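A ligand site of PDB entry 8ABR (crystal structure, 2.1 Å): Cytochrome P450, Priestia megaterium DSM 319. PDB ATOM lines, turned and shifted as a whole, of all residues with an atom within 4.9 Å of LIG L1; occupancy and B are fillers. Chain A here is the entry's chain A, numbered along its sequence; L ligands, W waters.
FE1 of LIG L1 is bound by SG of Cys 351 (2.2 Å).
A ring nitrogen (NE2) of His 91 lies within hydrogen-bond range of an oxygen (O3) of LIG L1.
A ring nitrogen (ND1) of His 349 lies within hydrogen-bond range of an oxygen (O4) of LIG L1 (2.7 Å).
NH1 of Arg 293 lies within salt-bridge range of O2 of LIG L1, at 2.8 Å.
The guanidinium group of Arg 95 lies within salt-bridge range of an oxygen (O3) of LIG L1, 2.8 Å away.
An oxygen (O2) of LIG L1 lies within salt-bridge range of the guanidinium group (NH2) of Arg 74 (3.0 Å).
An oxygen (O4) of LIG L1 lies close to the backbone NH of Leu 84 (3.5 Å).
NH2 of Arg 74 lies within salt-bridge range of O2 of LG2 L2.
SG of Cys 351 sits close to N of Gly 353, 3.3 Å away.
The guanidinium group (NE) of Arg 293 sits close to the side-chain hydroxyl (OG) of Ser 72, at 3.4 Å.
The guanidinium group (NH1) of Arg 95 lies within hydrogen-bond range of the backbone carbonyl oxygen (O) of Ile 348 (3.3 Å).
The backbone carbonyl oxygen of Phe 350 sits at hydrogen-bond distance from the guanidinium group of Arg 95, at 2.8 Å.
The backbone carbonyl oxygen of Leu 84 lies within hydrogen-bond range of the guanidinium group of Arg 74, 3.3 Å away.
NH1 of Arg 74 is in hydrogen-bond range of O of Ser 72 (3.0 Å).
OG1 of Thr 245 lies within hydrogen-bond range of O of Ala 241 (2.6 Å).
The backbone carbonyl oxygen (O) of Leu 282 is in hydrogen-bond range of the side-chain hydroxyl (OG) of Ser 343, 2.6 Å away.
The backbone carbonyl oxygen of Ile 83 lies close to an oxygen (O4) of LIG L1 (3.3 Å).
CE1 of Phe 102 touches C26 of LIG L1, at 3.9 Å.
Ile 146 touches LIG L1.
Leu 237 touches LIG L1.
Leu 238 touches LIG L1.
Ala 241 touches LIG L1 (O to C20, 3.6 Å).
Gly 242 touches LIG L1 (CA to C24, 3.6 Å).
Thr 245 touches LIG L1 (OG1 to C15, 3.2 Å).
OG1 of Thr 246 touches C24 of LIG L1 (3.7 Å).
Leu 249 touches LIG L1 (CD2 to C19, 3.96 Å).
Leu 282 touches LIG L1.
CB of Pro 287 touches C17 of LIG L1, at 3.8 Å.
Ile 288 touches LIG L1 (CG1 to C2, 3.9 Å).
Ile 291 touches LIG L1 (CG2 to C12, 3.5 Å).
Ser 343 touches LIG L1 (O to C9, 3.5 Å).
Phe 344 touches LIG L1 (C to C9, 3.6 Å).
N of Gly 345 touches C9 of LIG L1 (3.6 Å).
Ile 348 touches LIG L1.
Leu 352 touches LIG L1.
CA of Gly 353 touches C22 of LIG L1, 3.5 Å away.
Leu 356 touches LIG L1 (CD2 to C26, 3.6 Å).
Ala 357 touches LIG L1.
29 residues have an atom within 4 Å of LIG L1: Arg 74, Ile 83, Leu 84, His 91, Arg 95, Phe 102, Ile 146, Leu 237, Leu 238, Ala 241, Gly 242, Thr 245, Thr 246, Leu 249, Leu 282, Pro 287, Ile 288, Ile 291, Arg 293, Ser 343, Phe 344, Gly 345, Ile 348, His 349, Cys 351, Leu 352, Gly 353, Leu 356 and Ala 357.
Water W1 lies within hydrogen-bond range of O2 of LIG L1 (2.6 Å), O of Leu 84 (2.7 Å), OG of Ser 72 (2.7 Å), ND1 of His 349 (3.0 Å), NH1 of Arg 74 (3.1 Å) and NH1 of Arg 293 (3.3 Å).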
ATOM      1  N   LEU A  64      18.929 -36.432  -1.963  1.00  0.00           N
ATOM      2  CA  LEU A  64      18.943 -35.077  -2.504  1.00  0.00           C
ATOM      3  C   LEU A  64      19.006 -34.020  -1.404  1.00  0.00           C
ATOM      4  O   LEU A  64      19.585 -32.950  -1.608  1.00  0.00           O
ATOM      5  CB  LEU A  64      17.710 -34.846  -3.382  1.00  0.00           C
ATOM      6  CG  LEU A  64      17.534 -35.753  -4.583  1.00  0.00           C
ATOM      7  CD1 LEU A  64      16.240 -35.567  -5.357  1.00  0.00           C
ATOM      8  CD2 LEU A  64      18.728 -35.573  -5.536  1.00  0.00           C
ATOM      9  N   SER A  72      27.473 -33.770  -5.444  1.00  0.00           N
ATOM     10  CA  SER A  72      27.124 -33.555  -6.835  1.00  0.00           C
ATOM     11  C   SER A  72      28.350 -33.520  -7.745  1.00  0.00           C
ATOM     12  O   SER A  72      28.179 -33.333  -8.967  1.00  0.00           O
ATOM     13  CB  SER A  72      26.325 -32.250  -6.986  1.00  0.00           C
ATOM     14  OG  SER A  72      25.093 -32.326  -6.298  1.00  0.00           O
ATOM     15  N   ARG A  74      30.301 -35.093  -9.820  1.00  0.00           N
ATOM     16  CA  ARG A  74      30.245 -36.356 -10.549  1.00  0.00           C
ATOM     17  C   ARG A  74      30.666 -36.187 -12.002  1.00  0.00           C
ATOM     18  O   ARG A  74      30.354 -37.046 -12.835  1.00  0.00           O
ATOM     19  CB  ARG A  74      28.840 -36.958 -10.476  1.00  0.00           C
ATOM     20  CG  ARG A  74      27.739 -36.077 -11.124  1.00  0.00           C
ATOM     21  CD  ARG A  74      26.413 -36.374 -10.437  1.00  0.00           C
ATOM     22  NE  ARG A  74      25.242 -35.780 -11.055  1.00  0.00           N
ATOM     23  CZ  ARG A  74      24.703 -34.621 -10.689  1.00  0.00           C
ATOM     24  NH1 ARG A  74      25.324 -33.804  -9.855  1.00  0.00           N
ATOM     25  NH2 ARG A  74      23.507 -34.284 -11.160  1.00  0.00           N
ATOM     26  N   ILE A  83      27.180 -25.159 -11.920  1.00  0.00           N
ATOM     27  CA  ILE A  83      26.647 -25.363 -10.578  1.00  0.00           C
ATOM     28  C   ILE A  83      26.039 -26.744 -10.420  1.00  0.00           C
ATOM     29  O   ILE A  83      25.951 -27.262  -9.307  1.00  0.00           O
ATOM     30  CB  ILE A  83      25.618 -24.258 -10.242  1.00  0.00           C
ATOM     31  CG1 ILE A  83      24.518 -24.224 -11.309  1.00  0.00           C
ATOM     32  CG2 ILE A  83      26.294 -22.895 -10.173  1.00  0.00           C
ATOM     33  CD1 ILE A  83      23.352 -23.282 -10.938  1.00  0.00           C
ATOM     34  N   LEU A  84      25.584 -27.357 -11.507  1.00  0.00           N
ATOM     35  CA  LEU A  84      25.041 -28.707 -11.432  1.00  0.00           C
ATOM     36  C   LEU A  84      26.021 -29.668 -10.777  1.00  0.00           C
ATOM     37  O   LEU A  84      25.616 -30.556 -10.021  1.00  0.00           O
ATOM     38  CB  LEU A  84      24.692 -29.218 -12.829  1.00  0.00           C
ATOM     39  CG  LEU A  84      24.144 -30.645 -12.916  1.00  0.00           C
ATOM     40  CD1 LEU A  84      22.808 -30.731 -12.219  1.00  0.00           C
ATOM     41  CD2 LEU A  84      24.024 -31.118 -14.379  1.00  0.00           C
ATOM     42  N   HIS A  91      28.895 -23.848  -4.949  1.00  0.00           N
ATOM     43  CA  HIS A  91      27.576 -23.919  -5.567  1.00  0.00           C
ATOM     44  C   HIS A  91      26.701 -22.778  -5.084  1.00  0.00           C
ATOM     45  O   HIS A  91      25.956 -22.169  -5.869  1.00  0.00           O
ATOM     46  CB  HIS A  91      26.909 -25.242  -5.223  1.00  0.00           C
ATOM     47  CG  HIS A  91      25.465 -25.295  -5.602  1.00  0.00           C
ATOM     48  ND1 HIS A  91      24.444 -25.047  -4.689  1.00  0.00           N
ATOM     49  CD2 HIS A  91      24.847 -25.564  -6.783  1.00  0.00           C
ATOM     50  CE1 HIS A  91      23.275 -25.170  -5.292  1.00  0.00           C
ATOM     51  NE2 HIS A  91      23.494 -25.491  -6.558  1.00  0.00           N
ATOM     52  N   ARG A  95      25.200 -20.026  -7.729  1.00  0.00           N
ATOM     53  CA  ARG A  95      23.759 -20.048  -7.896  1.00  0.00           C
ATOM     54  C   ARG A  95      23.098 -18.757  -7.400  1.00  0.00           C
ATOM     55  O   ARG A  95      22.070 -18.347  -7.934  1.00  0.00           O
ATOM     56  CB  ARG A  95      23.158 -21.254  -7.173  1.00  0.00           C
ATOM     57  CG  ARG A  95      21.620 -21.291  -7.310  1.00  0.00           C
ATOM     58  CD  ARG A  95      21.004 -22.616  -6.931  1.00  0.00           C
ATOM     59  NE  ARG A  95      19.550 -22.508  -6.968  1.00  0.00           N
ATOM     60  CZ  ARG A  95      18.735 -23.459  -7.400  1.00  0.00           C
ATOM     61  NH1 ARG A  95      19.194 -24.602  -7.875  1.00  0.00           N
ATOM     62  NH2 ARG A  95      17.414 -23.271  -7.342  1.00  0.00           N
ATOM     63  N   PHE A 102      15.148 -16.342 -12.364  1.00  0.00           N
ATOM     64  CA  PHE A 102      14.278 -17.445 -12.773  1.00  0.00           C
ATOM     65  C   PHE A 102      13.095 -17.629 -11.840  1.00  0.00           C
ATOM     66  O   PHE A 102      12.448 -18.682 -11.864  1.00  0.00           O
ATOM     67  CB  PHE A 102      15.097 -18.734 -12.881  1.00  0.00           C
ATOM     68  CG  PHE A 102      16.186 -18.668 -13.915  1.00  0.00           C
ATOM     69  CD1 PHE A 102      15.908 -18.964 -15.232  1.00  0.00           C
ATOM     70  CD2 PHE A 102      17.467 -18.286 -13.570  1.00  0.00           C
ATOM     71  CE1 PHE A 102      16.898 -18.860 -16.206  1.00  0.00           C
ATOM     72  CE2 PHE A 102      18.468 -18.199 -14.513  1.00  0.00           C
ATOM     73  CZ  PHE A 102      18.186 -18.482 -15.841  1.00  0.00           C
ATOM     74  N   ILE A 146      15.034 -20.090 -24.418  1.00  0.00           N
ATOM     75  CA  ILE A 146      16.251 -20.040 -23.620  1.00  0.00           C
ATOM     76  C   ILE A 146      17.322 -19.214 -24.328  1.00  0.00           C
ATOM     77  O   ILE A 146      18.138 -18.545 -23.677  1.00  0.00           O
ATOM     78  CB  ILE A 146      16.744 -21.455 -23.279  1.00  0.00           C
ATOM     79  CG1 ILE A 146      17.766 -21.351 -22.148  1.00  0.00           C
ATOM     80  CG2 ILE A 146      17.348 -22.143 -24.489  1.00  0.00           C
ATOM     81  CD1 ILE A 146      17.175 -20.912 -20.808  1.00  0.00           C
ATOM     82  N   LEU A 237      25.092 -25.285 -19.552  1.00  0.00           N
ATOM     83  CA  LEU A 237      24.087 -25.919 -18.685  1.00  0.00           C
ATOM     84  C   LEU A 237      22.730 -25.289 -18.919  1.00  0.00           C
ATOM     85  O   LEU A 237      21.734 -25.979 -19.166  1.00  0.00           O
ATOM     86  CB  LEU A 237      24.491 -25.803 -17.215  1.00  0.00           C
ATOM     87  CG  LEU A 237      23.448 -26.170 -16.158  1.00  0.00           C
ATOM     88  CD1 LEU A 237      23.002 -27.626 -16.296  1.00  0.00           C
ATOM     89  CD2 LEU A 237      24.012 -25.900 -14.762  1.00  0.00           C
ATOM     90  N   LEU A 238      22.670 -23.952 -18.914  1.00  0.00           N
ATOM     91  CA  LEU A 238      21.392 -23.281 -19.110  1.00  0.00           C
ATOM     92  C   LEU A 238      20.810 -23.589 -20.478  1.00  0.00           C
ATOM     93  O   LEU A 238      19.592 -23.770 -20.604  1.00  0.00           O
ATOM     94  CB  LEU A 238      21.575 -21.772 -18.939  1.00  0.00           C
ATOM     95  CG  LEU A 238      21.690 -21.264 -17.505  1.00  0.00           C
ATOM     96  CD1 LEU A 238      22.051 -19.778 -17.477  1.00  0.00           C
ATOM     97  CD2 LEU A 238      20.408 -21.540 -16.724  1.00  0.00           C
ATOM     98  N   ALA A 241      19.872 -27.736 -20.365  1.00  0.00           N
ATOM     99  CA  ALA A 241      18.767 -27.942 -19.434  1.00  0.00           C
ATOM    100  C   ALA A 241      17.528 -27.187 -19.886  1.00  0.00           C
ATOM    101  O   ALA A 241      16.412 -27.702 -19.823  1.00  0.00           O
ATOM    102  CB  ALA A 241      19.170 -27.530 -18.013  1.00  0.00           C
ATOM    103  N   GLY A 242      17.699 -25.956 -20.342  1.00  0.00           N
ATOM    104  CA  GLY A 242      16.542 -25.173 -20.735  1.00  0.00           C
ATOM    105  C   GLY A 242      15.692 -25.727 -21.882  1.00  0.00           C
ATOM    106  O   GLY A 242      14.496 -25.454 -21.951  1.00  0.00           O
ATOM    107  N   THR A 245      14.966 -30.887 -21.725  1.00  0.00           N
ATOM    108  CA  THR A 245      13.945 -31.365 -20.808  1.00  0.00           C
ATOM    109  C   THR A 245      12.575 -30.821 -21.164  1.00  0.00           C
ATOM    110  O   THR A 245      11.578 -31.565 -21.191  1.00  0.00           O
ATOM    111  CB  THR A 245      14.344 -30.940 -19.396  1.00  0.00           C
ATOM    112  OG1 THR A 245      14.542 -29.515 -19.415  1.00  0.00           O
ATOM    113  CG2 THR A 245      15.616 -31.612 -18.930  1.00  0.00           C
ATOM    114  N   THR A 246      12.482 -29.522 -21.425  1.00  0.00           N
ATOM    115  CA  THR A 246      11.183 -28.915 -21.683  1.00  0.00           C
ATOM    116  C   THR A 246      10.559 -29.503 -22.938  1.00  0.00           C
ATOM    117  O   THR A 246       9.335 -29.640 -23.044  1.00  0.00           O
ATOM    118  CB  THR A 246      11.341 -27.403 -21.806  1.00  0.00           C
ATOM    119  OG1 THR A 246      12.085 -26.901 -20.691  1.00  0.00           O
ATOM    120  CG2 THR A 246       9.979 -26.715 -21.849  1.00  0.00           C
ATOM    121  N   LEU A 249       9.007 -32.644 -21.814  1.00  0.00           N
ATOM    122  CA  LEU A 249       7.774 -32.374 -21.083  1.00  0.00           C
ATOM    123  C   LEU A 249       6.609 -32.210 -22.045  1.00  0.00           C
ATOM    124  O   LEU A 249       5.554 -32.811 -21.866  1.00  0.00           O
ATOM    125  CB  LEU A 249       7.915 -31.133 -20.205  1.00  0.00           C
ATOM    126  CG  LEU A 249       6.643 -30.480 -19.656  1.00  0.00           C
ATOM    127  CD1 LEU A 249       5.876 -31.421 -18.756  1.00  0.00           C
ATOM    128  CD2 LEU A 249       6.985 -29.176 -18.887  1.00  0.00           C
ATOM    129  N   LEU A 282       4.955 -34.395 -15.597  1.00  0.00           N
ATOM    130  CA  LEU A 282       6.260 -34.482 -14.952  1.00  0.00           C
ATOM    131  C   LEU A 282       6.360 -35.686 -14.026  1.00  0.00           C
ATOM    132  O   LEU A 282       7.400 -36.360 -13.975  1.00  0.00           O
ATOM    133  CB  LEU A 282       6.534 -33.205 -14.160  1.00  0.00           C
ATOM    134  CG  LEU A 282       6.754 -31.943 -14.982  1.00  0.00           C
ATOM    135  CD1 LEU A 282       6.642 -30.678 -14.199  1.00  0.00           C
ATOM    136  CD2 LEU A 282       8.105 -31.981 -15.699  1.00  0.00           C
ATOM    137  N   PRO A 287      10.674 -36.081 -17.700  1.00  0.00           N
ATOM    138  CA  PRO A 287      11.799 -35.882 -18.650  1.00  0.00           C
ATOM    139  C   PRO A 287      13.138 -36.388 -18.145  1.00  0.00           C
ATOM    140  O   PRO A 287      13.914 -36.954 -18.925  1.00  0.00           O
ATOM    141  CB  PRO A 287      11.794 -34.363 -18.859  1.00  0.00           C
ATOM    142  CG  PRO A 287      10.334 -33.992 -18.704  1.00  0.00           C
ATOM    143  CD  PRO A 287       9.869 -34.853 -17.552  1.00  0.00           C
ATOM    144  N   ILE A 288      13.435 -36.186 -16.867  1.00  0.00           N
ATOM    145  CA  ILE A 288      14.652 -36.691 -16.234  1.00  0.00           C
ATOM    146  C   ILE A 288      14.241 -37.845 -15.330  1.00  0.00           C
ATOM    147  O   ILE A 288      13.428 -37.672 -14.416  1.00  0.00           O
ATOM    148  CB  ILE A 288      15.381 -35.602 -15.447  1.00  0.00           C
ATOM    149  CG1 ILE A 288      15.871 -34.470 -16.363  1.00  0.00           C
ATOM    150  CG2 ILE A 288      16.542 -36.210 -14.680  1.00  0.00           C
ATOM    151  CD1 ILE A 288      16.915 -34.864 -17.366  1.00  0.00           C
ATOM    152  N   ILE A 291      18.922 -39.154 -11.163  1.00  0.00           N
ATOM    153  CA  ILE A 291      19.816 -38.094 -10.742  1.00  0.00           C
ATOM    154  C   ILE A 291      20.995 -38.750 -10.034  1.00  0.00           C
ATOM    155  O   ILE A 291      20.808 -39.543  -9.094  1.00  0.00           O
ATOM    156  CB  ILE A 291      19.133 -37.088  -9.799  1.00  0.00           C
ATOM    157  CG1 ILE A 291      17.886 -36.473 -10.434  1.00  0.00           C
ATOM    158  CG2 ILE A 291      20.129 -35.994  -9.377  1.00  0.00           C
ATOM    159  CD1 ILE A 291      16.999 -35.700  -9.412  1.00  0.00           C
ATOM    160  N   ARG A 293      24.693 -38.931  -7.879  1.00  0.00           N
ATOM    161  CA  ARG A 293      25.390 -38.379  -6.738  1.00  0.00           C
ATOM    162  C   ARG A 293      26.583 -39.289  -6.472  1.00  0.00           C
ATOM    163  O   ARG A 293      26.620 -40.442  -6.910  1.00  0.00           O
ATOM    164  CB  ARG A 293      24.482 -38.303  -5.493  1.00  0.00           C
ATOM    165  CG  ARG A 293      23.385 -37.247  -5.546  1.00  0.00           C
ATOM    166  CD  ARG A 293      23.969 -35.832  -5.546  1.00  0.00           C
ATOM    167  NE  ARG A 293      22.937 -34.817  -5.332  1.00  0.00           N
ATOM    168  CZ  ARG A 293      22.283 -34.193  -6.308  1.00  0.00           C
ATOM    169  NH1 ARG A 293      22.496 -34.500  -7.575  1.00  0.00           N
ATOM    170  NH2 ARG A 293      21.395 -33.253  -6.009  1.00  0.00           N
ATOM    171  N   VAL A 342       9.459 -35.612  -7.698  1.00  0.00           N
ATOM    172  CA  VAL A 342      10.843 -35.151  -7.614  1.00  0.00           C
ATOM    173  C   VAL A 342      11.435 -35.002  -8.999  1.00  0.00           C
ATOM    174  O   VAL A 342      12.650 -35.161  -9.188  1.00  0.00           O
ATOM    175  CB  VAL A 342      11.705 -36.084  -6.749  1.00  0.00           C
ATOM    176  CG1 VAL A 342      11.357 -35.903  -5.315  1.00  0.00           C
ATOM    177  CG2 VAL A 342      11.515 -37.535  -7.142  1.00  0.00           C
ATOM    178  N   SER A 343      10.580 -34.673  -9.979  1.00  0.00           N
ATOM    179  CA  SER A 343      11.053 -34.519 -11.357  1.00  0.00           C
ATOM    180  C   SER A 343      11.919 -33.286 -11.560  1.00  0.00           C
ATOM    181  O   SER A 343      12.645 -33.191 -12.551  1.00  0.00           O
ATOM    182  CB  SER A 343       9.851 -34.461 -12.283  1.00  0.00           C
ATOM    183  OG  SER A 343       9.037 -35.605 -12.114  1.00  0.00           O
ATOM    184  N   PHE A 344      11.882 -32.330 -10.642  1.00  0.00           N
ATOM    185  CA  PHE A 344      12.801 -31.205 -10.640  1.00  0.00           C
ATOM    186  C   PHE A 344      13.894 -31.365  -9.595  1.00  0.00           C
ATOM    187  O   PHE A 344      14.594 -30.381  -9.294  1.00  0.00           O
ATOM    188  CB  PHE A 344      12.019 -29.918 -10.368  1.00  0.00           C
ATOM    189  CG  PHE A 344      11.183 -29.458 -11.525  1.00  0.00           C
ATOM    190  CD1 PHE A 344      11.732 -29.276 -12.784  1.00  0.00           C
ATOM    191  CD2 PHE A 344       9.832 -29.156 -11.339  1.00  0.00           C
ATOM    192  CE1 PHE A 344      10.950 -28.844 -13.836  1.00  0.00           C
ATOM    193  CE2 PHE A 344       9.056 -28.714 -12.409  1.00  0.00           C
ATOM    194  CZ  PHE A 344       9.628 -28.553 -13.657  1.00  0.00           C
ATOM    195  N   GLY A 345      14.032 -32.558  -9.007  1.00  0.00           N
ATOM    196  CA  GLY A 345      14.968 -32.742  -7.908  1.00  0.00           C
ATOM    197  C   GLY A 345      14.403 -32.248  -6.594  1.00  0.00           C
ATOM    198  O   GLY A 345      13.195 -32.057  -6.445  1.00  0.00           O
ATOM    199  N   ILE A 348      19.056 -28.144  -2.478  1.00  0.00           N
ATOM    200  CA  ILE A 348      19.818 -26.985  -2.934  1.00  0.00           C
ATOM    201  C   ILE A 348      20.035 -26.978  -4.440  1.00  0.00           C
ATOM    202  O   ILE A 348      20.267 -25.908  -5.001  1.00  0.00           O
ATOM    203  CB  ILE A 348      21.176 -26.902  -2.222  1.00  0.00           C
ATOM    204  CG1 ILE A 348      22.024 -28.140  -2.507  1.00  0.00           C
ATOM    205  CG2 ILE A 348      20.991 -26.728  -0.712  1.00  0.00           C
ATOM    206  CD1 ILE A 348      23.451 -28.057  -1.939  1.00  0.00           C
ATOM    207  N   HIS A 349      19.965 -28.129  -5.110  1.00  0.00           N
ATOM    208  CA  HIS A 349      20.108 -28.181  -6.563  1.00  0.00           C
ATOM    209  C   HIS A 349      18.764 -28.182  -7.293  1.00  0.00           C
ATOM    210  O   HIS A 349      18.715 -28.327  -8.516  1.00  0.00           O
ATOM    211  CB  HIS A 349      20.933 -29.402  -6.991  1.00  0.00           C
ATOM    212  CG  HIS A 349      22.383 -29.318  -6.642  1.00  0.00           C
ATOM    213  ND1 HIS A 349      23.332 -28.759  -7.475  1.00  0.00           N
ATOM    214  CD2 HIS A 349      23.053 -29.717  -5.531  1.00  0.00           C
ATOM    215  CE1 HIS A 349      24.527 -28.840  -6.902  1.00  0.00           C
ATOM    216  NE2 HIS A 349      24.380 -29.403  -5.715  1.00  0.00           N
ATOM    217  N   PHE A 350      17.660 -28.020  -6.560  1.00  0.00           N
ATOM    218  CA  PHE A 350      16.333 -28.002  -7.168  1.00  0.00           C
ATOM    219  C   PHE A 350      16.321 -27.132  -8.419  1.00  0.00           C
ATOM    220  O   PHE A 350      16.846 -26.016  -8.427  1.00  0.00           O
ATOM    221  CB  PHE A 350      15.298 -27.481  -6.164  1.00  0.00           C
ATOM    222  CG  PHE A 350      13.889 -27.509  -6.690  1.00  0.00           C
ATOM    223  CD1 PHE A 350      13.134 -28.672  -6.635  1.00  0.00           C
ATOM    224  CD2 PHE A 350      13.313 -26.364  -7.232  1.00  0.00           C
ATOM    225  CE1 PHE A 350      11.842 -28.696  -7.119  1.00  0.00           C
ATOM    226  CE2 PHE A 350      12.031 -26.392  -7.715  1.00  0.00           C
ATOM    227  CZ  PHE A 350      11.292 -27.541  -7.659  1.00  0.00           C
ATOM    228  N   CYS A 351      15.716 -27.651  -9.470  1.00  0.00           N
ATOM    229  CA  CYS A 351      15.722 -27.067 -10.792  1.00  0.00           C
ATOM    230  C   CYS A 351      15.543 -25.551 -10.798  1.00  0.00           C
ATOM    231  O   CYS A 351      14.533 -25.023 -10.344  1.00  0.00           O
ATOM    232  CB  CYS A 351      14.618 -27.683 -11.613  1.00  0.00           C
ATOM    233  SG  CYS A 351      14.702 -27.004 -13.318  1.00  0.00           S
ATOM    234  N   LEU A 352      16.534 -24.842 -11.304  1.00  0.00           N
ATOM    235  CA  LEU A 352      16.444 -23.382 -11.342  1.00  0.00           C
ATOM    236  C   LEU A 352      15.382 -22.902 -12.332  1.00  0.00           C
ATOM    237  O   LEU A 352      14.768 -21.855 -12.135  1.00  0.00           O
ATOM    238  CB  LEU A 352      17.804 -22.801 -11.722  1.00  0.00           C
ATOM    239  CG  LEU A 352      18.106 -21.351 -11.358  1.00  0.00           C
ATOM    240  CD1 LEU A 352      18.376 -21.213  -9.872  1.00  0.00           C
ATOM    241  CD2 LEU A 352      19.278 -20.894 -12.240  1.00  0.00           C
ATOM    242  N   GLY A 353      15.130 -23.689 -13.359  1.00  0.00           N
ATOM    243  CA  GLY A 353      14.188 -23.322 -14.387  1.00  0.00           C
ATOM    244  C   GLY A 353      12.778 -23.807 -14.203  1.00  0.00           C
ATOM    245  O   GLY A 353      11.999 -23.707 -15.146  1.00  0.00           O
ATOM    246  N   LEU A 356      10.026 -21.483 -15.259  1.00  0.00           N
ATOM    247  CA  LEU A 356      10.014 -21.308 -16.707  1.00  0.00           C
ATOM    248  C   LEU A 356       9.496 -22.552 -17.423  1.00  0.00           C
ATOM    249  O   LEU A 356       8.702 -22.435 -18.377  1.00  0.00           O
ATOM    250  CB  LEU A 356      11.419 -20.925 -17.173  1.00  0.00           C
ATOM    251  CG  LEU A 356      11.552 -20.569 -18.665  1.00  0.00           C
ATOM    252  CD1 LEU A 356      10.669 -19.383 -19.007  1.00  0.00           C
ATOM    253  CD2 LEU A 356      13.014 -20.259 -19.016  1.00  0.00           C
ATOM    254  N   ALA A 357       9.963 -23.731 -17.032  1.00  0.00           N
ATOM    255  CA  ALA A 357       9.454 -24.953 -17.627  1.00  0.00           C
ATOM    256  C   ALA A 357       7.952 -25.064 -17.449  1.00  0.00           C
ATOM    257  O   ALA A 357       7.245 -25.483 -18.369  1.00  0.00           O
ATOM    258  CB  ALA A 357      10.156 -26.166 -16.992  1.00  0.00           C
ATOM    259  N   GLU A 360       6.230 -22.646 -19.837  1.00  0.00           N
ATOM    260  CA  GLU A 360       6.297 -23.124 -21.222  1.00  0.00           C
ATOM    261  C   GLU A 360       5.367 -24.299 -21.446  1.00  0.00           C
ATOM    262  O   GLU A 360       4.656 -24.364 -22.464  1.00  0.00           O
ATOM    263  CB  GLU A 360       7.731 -23.506 -21.601  1.00  0.00           C
ATOM    264  CG  GLU A 360       8.710 -22.315 -21.693  1.00  0.00           C
ATOM    265  CD  GLU A 360      10.130 -22.711 -22.094  1.00  0.00           C
ATOM    266  OE1 GLU A 360      10.239 -23.590 -22.974  1.00  0.00           O
ATOM    267  OE2 GLU A 360      11.086 -22.149 -21.550  1.00  0.00           O
HETATM  268 FE1  LIG L   1      16.264 -28.013 -14.574  1.00  0.00          FE
HETATM  269  C1  LIG L   1      18.580 -28.642 -12.141  1.00  0.00           C
HETATM  270  C2  LIG L   1      15.078 -31.186 -14.317  1.00  0.00           C
HETATM  271  C3  LIG L   1      13.926 -27.371 -17.069  1.00  0.00           C
HETATM  272  C4  LIG L   1      17.960 -25.181 -15.494  1.00  0.00           C
HETATM  273  N1  LIG L   1      16.769 -29.611 -13.479  1.00  0.00           N
HETATM  274  C5  LIG L   1      17.670 -29.659 -12.433  1.00  0.00           C
HETATM  275  C6  LIG L   1      17.531 -30.928 -11.693  1.00  0.00           C
HETATM  276  C7  LIG L   1      16.548 -31.595 -12.301  1.00  0.00           C
HETATM  277  C8  LIG L   1      16.083 -30.792 -13.438  1.00  0.00           C
HETATM  278  C9  LIG L   1      16.038 -33.006 -11.932  1.00  0.00           C
HETATM  279  C10 LIG L   1      18.322 -31.364 -10.419  1.00  0.00           C
HETATM  280  C11 LIG L   1      19.565 -32.203 -10.691  1.00  0.00           C
HETATM  281  C12 LIG L   1      20.363 -32.469  -9.426  1.00  0.00           C
HETATM  282  O1  LIG L   1      19.785 -32.522  -8.319  1.00  0.00           O
HETATM  283  O2  LIG L   1      21.611 -32.635  -9.531  1.00  0.00           O
HETATM  284  N2  LIG L   1      14.817 -29.096 -15.564  1.00  0.00           N
HETATM  285  C13 LIG L   1      14.443 -30.377 -15.250  1.00  0.00           C
HETATM  286  C14 LIG L   1      13.230 -30.714 -15.980  1.00  0.00           C
HETATM  287  C15 LIG L   1      12.919 -29.658 -16.717  1.00  0.00           C
HETATM  288  C16 LIG L   1      13.886 -28.612 -16.429  1.00  0.00           C
HETATM  289  C17 LIG L   1      12.462 -32.057 -15.908  1.00  0.00           C
HETATM  290  C18 LIG L   1      11.755 -29.441 -17.689  1.00  0.00           C
HETATM  291  C19 LIG L   1      10.589 -30.017 -17.490  1.00  0.00           C
HETATM  292  N3  LIG L   1      16.026 -26.647 -16.055  1.00  0.00           N
HETATM  293  C20 LIG L   1      14.908 -26.435 -16.851  1.00  0.00           C
HETATM  294  C21 LIG L   1      14.956 -25.122 -17.479  1.00  0.00           C
HETATM  295  C22 LIG L   1      16.078 -24.527 -17.038  1.00  0.00           C
HETATM  296  C23 LIG L   1      16.746 -25.446 -16.133  1.00  0.00           C
HETATM  297  C24 LIG L   1      13.868 -24.568 -18.440  1.00  0.00           C
HETATM  298  C25 LIG L   1      16.637 -23.108 -17.322  1.00  0.00           C
HETATM  299  C26 LIG L   1      15.914 -22.211 -17.981  1.00  0.00           C
HETATM  300  N4  LIG L   1      17.961 -27.082 -13.901  1.00  0.00           N
HETATM  301  C27 LIG L   1      18.502 -25.956 -14.470  1.00  0.00           C
HETATM  302  C28 LIG L   1      19.761 -25.701 -13.776  1.00  0.00           C
HETATM  303  C29 LIG L   1      19.944 -26.658 -12.861  1.00  0.00           C
HETATM  304  C30 LIG L   1      18.817 -27.541 -12.932  1.00  0.00           C
HETATM  305  C31 LIG L   1      20.722 -24.533 -14.122  1.00  0.00           C
HETATM  306  C32 LIG L   1      21.131 -26.766 -11.886  1.00  0.00           C
HETATM  307  C33 LIG L   1      20.736 -26.140 -10.514  1.00  0.00           C
HETATM  308  C34 LIG L   1      21.777 -26.398  -9.465  1.00  0.00           C
HETATM  309  O3  LIG L   1      21.766 -25.709  -8.405  1.00  0.00           O
HETATM  310  O4  LIG L   1      22.629 -27.294  -9.667  1.00  0.00           O
HETATM  311  C1  LG2 L   2      21.174 -35.416 -14.634  1.00  0.00           C
HETATM  312  C2  LG2 L   2      22.147 -36.315 -13.868  1.00  0.00           C
HETATM  313  O1  LG2 L   2      22.981 -36.944 -14.511  1.00  0.00           O
HETATM  314  C3  LG2 L   2      20.254 -34.511 -13.816  1.00  0.00           C
HETATM  315  C4  LG2 L   2      19.483 -33.550 -14.711  1.00  0.00           C
HETATM  316  C5  LG2 L   2      20.004 -32.120 -14.677  1.00  0.00           C
HETATM  317  C6  LG2 L   2      19.274 -31.214 -15.669  1.00  0.00           C
HETATM  318  O2  LG2 L   2      22.025 -36.338 -12.614  1.00  0.00           O
HETATM  319  O   HOH W   1      23.677 -31.563  -8.457  1.00  0.00           O
HETATM  320  O   HOH W   2      17.822 -31.653  -6.582  1.00  0.00           O
